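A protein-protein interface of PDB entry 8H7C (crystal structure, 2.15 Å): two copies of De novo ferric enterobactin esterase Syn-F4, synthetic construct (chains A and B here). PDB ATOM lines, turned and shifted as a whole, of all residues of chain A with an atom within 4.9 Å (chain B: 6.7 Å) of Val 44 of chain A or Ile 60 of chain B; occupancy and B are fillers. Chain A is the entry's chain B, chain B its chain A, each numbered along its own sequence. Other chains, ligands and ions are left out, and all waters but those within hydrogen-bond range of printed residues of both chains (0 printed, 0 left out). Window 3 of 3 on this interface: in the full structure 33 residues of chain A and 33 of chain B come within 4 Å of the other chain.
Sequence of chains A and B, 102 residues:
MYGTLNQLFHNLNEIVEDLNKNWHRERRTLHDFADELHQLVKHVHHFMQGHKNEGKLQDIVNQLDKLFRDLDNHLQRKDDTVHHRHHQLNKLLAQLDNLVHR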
ATOM      1  N   LEU A  40      23.874 -11.747 -25.923  1.00  0.00           N
ATOM      2  CA  LEU A  40      24.786 -12.875 -26.004  1.00  0.00           C
ATOM      3  C   LEU A  40      26.235 -12.426 -26.187  1.00  0.00           C
ATOM      4  O   LEU A  40      27.138 -13.060 -25.660  1.00  0.00           O
ATOM      5  CB  LEU A  40      24.365 -13.773 -27.169  1.00  0.00           C
ATOM      6  CG  LEU A  40      25.114 -15.090 -27.368  1.00  0.00           C
ATOM      7  CD1 LEU A  40      24.626 -16.138 -26.390  1.00  0.00           C
ATOM      8  CD2 LEU A  40      24.913 -15.581 -28.782  1.00  0.00           C
ATOM      9  N   VAL A  41      26.450 -11.352 -26.950  1.00  0.00           N
ATOM     10  CA  VAL A  41      27.787 -10.771 -27.122  1.00  0.00           C
ATOM     11  C   VAL A  41      28.263 -10.226 -25.781  1.00  0.00           C
ATOM     12  O   VAL A  41      29.292 -10.662 -25.276  1.00  0.00           O
ATOM     13  CB  VAL A  41      27.819  -9.667 -28.213  1.00  0.00           C
ATOM     14  CG1 VAL A  41      29.123  -8.869 -28.181  1.00  0.00           C
ATOM     15  CG2 VAL A  41      27.646 -10.291 -29.588  1.00  0.00           C
ATOM     16  N   LYS A  42      27.504  -9.281 -25.225  1.00  0.00           N
ATOM     17  CA  LYS A  42      27.717  -8.765 -23.864  1.00  0.00           C
ATOM     18  C   LYS A  42      28.063  -9.880 -22.881  1.00  0.00           C
ATOM     19  O   LYS A  42      29.050  -9.793 -22.154  1.00  0.00           O
ATOM     20  CB  LYS A  42      26.453  -8.070 -23.334  1.00  0.00           C
ATOM     21  CG  LYS A  42      26.170  -6.674 -23.863  1.00  0.00           C
ATOM     22  CD  LYS A  42      24.977  -6.090 -23.117  1.00  0.00           C
ATOM     23  CE  LYS A  42      24.622  -4.685 -23.576  1.00  0.00           C
ATOM     24  NZ  LYS A  42      23.696  -4.704 -24.736  1.00  0.00           N
ATOM     25  N   HIS A  43      27.244 -10.925 -22.882  1.00  0.00           N
ATOM     26  CA  HIS A  43      27.373 -12.017 -21.928  1.00  0.00           C
ATOM     27  C   HIS A  43      28.690 -12.776 -22.064  1.00  0.00           C
ATOM     28  O   HIS A  43      29.401 -12.949 -21.082  1.00  0.00           O
ATOM     29  CB  HIS A  43      26.196 -12.974 -22.063  1.00  0.00           C
ATOM     30  CG  HIS A  43      26.355 -14.242 -21.283  1.00  0.00           C
ATOM     31  ND1 HIS A  43      26.109 -14.324 -19.928  1.00  0.00           N
ATOM     32  CD2 HIS A  43      26.743 -15.482 -21.670  1.00  0.00           C
ATOM     33  CE1 HIS A  43      26.332 -15.561 -19.517  1.00  0.00           C
ATOM     34  NE2 HIS A  43      26.719 -16.282 -20.553  1.00  0.00           N
ATOM     35  N   VAL A  44      29.006 -13.220 -23.276  1.00  0.00           N
ATOM     36  CA  VAL A  44      30.249 -13.968 -23.565  1.00  0.00           C
ATOM     37  C   VAL A  44      31.512 -13.133 -23.271  1.00  0.00           C
ATOM     38  O   VAL A  44      32.549 -13.681 -22.891  1.00  0.00           O
ATOM     39  CB  VAL A  44      30.245 -14.515 -25.019  1.00  0.00           C
ATOM     40  CG1 VAL A  44      31.587 -15.117 -25.421  1.00  0.00           C
ATOM     41  CG2 VAL A  44      29.168 -15.576 -25.175  1.00  0.00           C
ATOM     42  N   HIS A  45      31.417 -11.816 -23.440  1.00  0.00           N
ATOM     43  CA  HIS A  45      32.438 -10.888 -22.942  1.00  0.00           C
ATOM     44  C   HIS A  45      32.613 -10.981 -21.406  1.00  0.00           C
ATOM     45  O   HIS A  45      33.715 -10.797 -20.897  1.00  0.00           O
ATOM     46  CB  HIS A  45      32.088  -9.451 -23.349  1.00  0.00           C
ATOM     47  CG  HIS A  45      33.231  -8.496 -23.223  1.00  0.00           C
ATOM     48  ND1 HIS A  45      34.022  -8.140 -24.292  1.00  0.00           N
ATOM     49  CD2 HIS A  45      33.726  -7.837 -22.149  1.00  0.00           C
ATOM     50  CE1 HIS A  45      34.953  -7.294 -23.884  1.00  0.00           C
ATOM     51  NE2 HIS A  45      34.796  -7.096 -22.588  1.00  0.00           N
ATOM     52  N   HIS A  46      31.508 -11.267 -20.709  1.00  0.00           N
ATOM     53  CA  HIS A  46      31.403 -11.430 -19.230  1.00  0.00           C
ATOM     54  C   HIS A  46      32.079 -10.326 -18.396  1.00  0.00           C
ATOM     55  O   HIS A  46      31.414  -9.592 -17.660  1.00  0.00           O
ATOM     56  CB  HIS A  46      31.737 -12.859 -18.716  1.00  0.00           C
ATOM     57  CG  HIS A  46      33.092 -13.377 -19.098  1.00  0.00           C
ATOM     58  ND1 HIS A  46      34.264 -12.697 -18.834  1.00  0.00           N
ATOM     59  CD2 HIS A  46      33.461 -14.547 -19.674  1.00  0.00           C
ATOM     60  CE1 HIS A  46      35.292 -13.409 -19.261  1.00  0.00           C
ATOM     61  NE2 HIS A  46      34.831 -14.537 -19.774  1.00  0.00           N
ATOM     62  N   LEU A  57      38.281 -18.968 -28.026  1.00  0.00           N
ATOM     63  CA  LEU A  57      37.146 -18.346 -27.330  1.00  0.00           C
ATOM     64  C   LEU A  57      36.996 -16.875 -27.726  1.00  0.00           C
ATOM     65  O   LEU A  57      35.887 -16.401 -27.955  1.00  0.00           O
ATOM     66  CB  LEU A  57      37.281 -18.465 -25.806  1.00  0.00           C
ATOM     67  CG  LEU A  57      35.982 -18.768 -25.032  1.00  0.00           C
ATOM     68  CD1 LEU A  57      36.283 -18.984 -23.553  1.00  0.00           C
ATOM     69  CD2 LEU A  57      34.904 -17.707 -25.191  1.00  0.00           C
ATOM     70  N   VAL A  61      34.029 -14.313 -29.703  1.00  0.00           N
ATOM     71  CA  VAL A  61      33.424 -12.988 -29.388  1.00  0.00           C
ATOM     72  C   VAL A  61      33.576 -11.999 -30.557  1.00  0.00           C
ATOM     73  O   VAL A  61      32.726 -11.128 -30.756  1.00  0.00           O
ATOM     74  CB  VAL A  61      33.982 -12.363 -28.074  1.00  0.00           C
ATOM     75  CG1 VAL A  61      35.452 -11.975 -28.196  1.00  0.00           C
ATOM     76  CG2 VAL A  61      33.168 -11.147 -27.638  1.00  0.00           C
ATOM     77  N   LEU A  64      31.016 -13.089 -33.183  1.00  0.00           N
ATOM     78  CA  LEU A  64      29.706 -12.605 -32.750  1.00  0.00           C
ATOM     79  C   LEU A  64      29.481 -11.095 -32.869  1.00  0.00           C
ATOM     80  O   LEU A  64      28.409 -10.662 -33.306  1.00  0.00           O
ATOM     81  CB  LEU A  64      29.452 -13.020 -31.302  1.00  0.00           C
ATOM     82  CG  LEU A  64      29.259 -14.502 -31.041  1.00  0.00           C
ATOM     83  CD1 LEU A  64      29.154 -14.733 -29.547  1.00  0.00           C
ATOM     84  CD2 LEU A  64      28.009 -14.996 -31.739  1.00  0.00           C
ATOM     85  N   VAL B  44      31.774 -23.255 -31.921  1.00  0.00           N
ATOM     86  CA  VAL B  44      31.590 -23.261 -30.459  1.00  0.00           C
ATOM     87  C   VAL B  44      31.346 -24.695 -29.956  1.00  0.00           C
ATOM     88  O   VAL B  44      31.788 -25.063 -28.868  1.00  0.00           O
ATOM     89  CB  VAL B  44      30.419 -22.345 -30.011  1.00  0.00           C
ATOM     90  CG1 VAL B  44      30.225 -22.375 -28.499  1.00  0.00           C
ATOM     91  CG2 VAL B  44      30.661 -20.905 -30.427  1.00  0.00           C
ATOM     92  N   LEU B  57      28.083 -22.545 -19.028  1.00  0.00           N
ATOM     93  CA  LEU B  57      29.299 -22.629 -19.846  1.00  0.00           C
ATOM     94  C   LEU B  57      29.025 -22.857 -21.339  1.00  0.00           C
ATOM     95  O   LEU B  57      29.610 -22.194 -22.200  1.00  0.00           O
ATOM     96  CB  LEU B  57      30.227 -23.732 -19.299  1.00  0.00           C
ATOM     97  CG  LEU B  57      29.961 -25.241 -19.483  1.00  0.00           C
ATOM     98  CD1 LEU B  57      31.214 -26.034 -19.121  1.00  0.00           C
ATOM     99  CD2 LEU B  57      28.770 -25.728 -18.664  1.00  0.00           C
ATOM    100  N   GLN B  58      28.137 -23.818 -21.599  1.00  0.00           N
ATOM    101  CA  GLN B  58      27.704 -24.272 -22.930  1.00  0.00           C
ATOM    102  C   GLN B  58      26.189 -23.954 -23.161  1.00  0.00           C
ATOM    103  O   GLN B  58      25.552 -24.401 -24.120  1.00  0.00           O
ATOM    104  CB  GLN B  58      28.068 -25.765 -23.036  1.00  0.00           C
ATOM    105  CG  GLN B  58      27.390 -26.605 -24.099  1.00  0.00           C
ATOM    106  CD  GLN B  58      26.216 -27.431 -23.579  1.00  0.00           C
ATOM    107  OE1 GLN B  58      25.429 -26.966 -22.742  1.00  0.00           O
ATOM    108  NE2 GLN B  58      26.093 -28.670 -24.075  1.00  0.00           N
ATOM    109  N   ASP B  59      25.636 -23.147 -22.263  1.00  0.00           N
ATOM    110  CA  ASP B  59      24.385 -22.422 -22.470  1.00  0.00           C
ATOM    111  C   ASP B  59      24.480 -21.514 -23.712  1.00  0.00           C
ATOM    112  O   ASP B  59      23.472 -21.187 -24.345  1.00  0.00           O
ATOM    113  CB  ASP B  59      24.118 -21.583 -21.213  1.00  0.00           C
ATOM    114  CG  ASP B  59      22.792 -20.872 -21.241  1.00  0.00           C
ATOM    115  OD1 ASP B  59      21.784 -21.471 -21.681  1.00  0.00           O
ATOM    116  OD2 ASP B  59      22.762 -19.703 -20.804  1.00  0.00           O
ATOM    117  N   ILE B  60      25.704 -21.100 -24.031  1.00  0.00           N
ATOM    118  CA  ILE B  60      26.018 -20.338 -25.232  1.00  0.00           C
ATOM    119  C   ILE B  60      25.725 -21.123 -26.529  1.00  0.00           C
ATOM    120  O   ILE B  60      25.162 -20.558 -27.467  1.00  0.00           O
ATOM    121  CB  ILE B  60      27.475 -19.817 -25.132  1.00  0.00           C
ATOM    122  CG1 ILE B  60      27.562 -18.770 -24.015  1.00  0.00           C
ATOM    123  CG2 ILE B  60      27.962 -19.177 -26.425  1.00  0.00           C
ATOM    124  CD1 ILE B  60      28.903 -18.732 -23.325  1.00  0.00           C
ATOM    125  N   VAL B  61      26.081 -22.406 -26.575  1.00  0.00           N
ATOM    126  CA  VAL B  61      25.713 -23.270 -27.717  1.00  0.00           C
ATOM    127  C   VAL B  61      24.188 -23.313 -27.938  1.00  0.00           C
ATOM    128  O   VAL B  61      23.727 -23.304 -29.083  1.00  0.00           O
ATOM    129  CB  VAL B  61      26.263 -24.707 -27.556  1.00  0.00           C
ATOM    130  CG1 VAL B  61      25.692 -25.671 -28.599  1.00  0.00           C
ATOM    131  CG2 VAL B  61      27.776 -24.692 -27.673  1.00  0.00           C
ATOM    132  N   ASN B  62      23.432 -23.356 -26.839  1.00  0.00           N
ATOM    133  CA  ASN B  62      21.969 -23.418 -26.873  1.00  0.00           C
ATOM    134  C   ASN B  62      21.324 -22.125 -27.360  1.00  0.00           C
ATOM    135  O   ASN B  62      20.412 -22.157 -28.177  1.00  0.00           O
ATOM    136  CB  ASN B  62      21.420 -23.767 -25.485  1.00  0.00           C
ATOM    137  CG  ASN B  62      21.615 -25.237 -25.116  1.00  0.00           C
ATOM    138  OD1 ASN B  62      22.123 -26.045 -25.906  1.00  0.00           O
ATOM    139  ND2 ASN B  62      21.200 -25.589 -23.903  1.00  0.00           N
ATOM    140  N   GLN B  63      21.799 -20.999 -26.837  1.00  0.00           N
ATOM    141  CA  GLN B  63      21.390 -19.668 -27.316  1.00  0.00           C
ATOM    142  C   GLN B  63      21.694 -19.490 -28.822  1.00  0.00           C
ATOM    143  O   GLN B  63      20.841 -19.072 -29.613  1.00  0.00           O
ATOM    144  CB  GLN B  63      22.082 -18.563 -26.499  1.00  0.00           C
ATOM    145  CG  GLN B  63      21.314 -18.067 -25.269  1.00  0.00           C
ATOM    146  CD  GLN B  63      22.231 -17.457 -24.202  1.00  0.00           C
ATOM    147  OE1 GLN B  63      22.385 -16.230 -24.104  1.00  0.00           O
ATOM    148  NE2 GLN B  63      22.855 -18.321 -23.400  1.00  0.00           N
ATOM    149  N   LEU B  64      22.921 -19.819 -29.200  1.00  0.00           N
ATOM    150  CA  LEU B  64      23.346 -19.760 -30.598  1.00  0.00           C
ATOM    151  C   LEU B  64      22.548 -20.681 -31.515  1.00  0.00           C
ATOM    152  O   LEU B  64      22.180 -20.279 -32.620  1.00  0.00           O
ATOM    153  CB  LEU B  64      24.836 -20.096 -30.723  1.00  0.00           C
ATOM    154  CG  LEU B  64      25.843 -19.032 -30.303  1.00  0.00           C
ATOM    155  CD1 LEU B  64      27.239 -19.610 -30.425  1.00  0.00           C
ATOM    156  CD2 LEU B  64      25.698 -17.796 -31.171  1.00  0.00           C
ATOM    157  N   ASP B  65      22.290 -21.906 -31.066  1.00  0.00           N
ATOM    158  CA  ASP B  65      21.497 -22.845 -31.862  1.00  0.00           C
ATOM    159  C   ASP B  65      20.030 -22.369 -32.022  1.00  0.00           C
ATOM    160  O   ASP B  65      19.403 -22.584 -33.068  1.00  0.00           O
ATOM    161  CB  ASP B  65      21.560 -24.259 -31.268  1.00  0.00           C
ATOM    162  CG  ASP B  65      21.104 -25.334 -32.259  1.00  0.00           C
ATOM    163  OD1 ASP B  65      21.480 -25.269 -33.459  1.00  0.00           O
ATOM    164  OD2 ASP B  65      20.367 -26.252 -31.836  1.00  0.00           O
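Hydrophobic or aromatic side chains of chain B that line the printed part of chain A: Ile 60 and Leu 64.
Of the 10 printed residues of chain A, 3 touch a printed residue of chain B.
Among the printed residues, 4 pairs touch across the chains.
Leu 40 of chain A touches Gln 63 of chain B (CD1 to OE1, 3.2 Å).
Leu 40 of chain A touches Leu 64 of chain B (CD2 to CD2, 3.4 Å).
Val 44 of chain A touches Ile 60 of chain B (CG2 to CD1, 3.7 Å).
CD2 of Leu 64 of chain A touches CD2 of Leu 64 of chain B (3.7 Å).
Leu 64 of chain B touches its own counterpart, Leu 64 of chain A.
4 positions are printed for both chains.
Ile 60 of chain B touches one residue of chain A.
Printed residues of chain A within 4 Å of Gln 63 of chain B: Leu 40 (3.2 Å).
Printed residues of chain B within 4 Å of Leu 40 of chain A: Gln 63 (3.2 Å) and Leu 64 (3.4 Å).
Of the printed residues of chain A, Leu 64 of chain B touches Leu 40 and Leu 64.
The nearest printed residue of chain B that does not touch Val 44 of chain A is Leu 64 of chain B (6.9 Å).
The nearest residue of chain A that does not touch Ile 60 of chain B is His 43 of chain A (4.1 Å).
The nearest printed residue of chain B that does not touch Leu 64 of chain A is Ile 60 of chain B (5.6 Å).
NE2 of Gln 63 of chain B sits at hydrogen-bond distance from OD2 of Asp 59 of chain B (2.9 Å).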
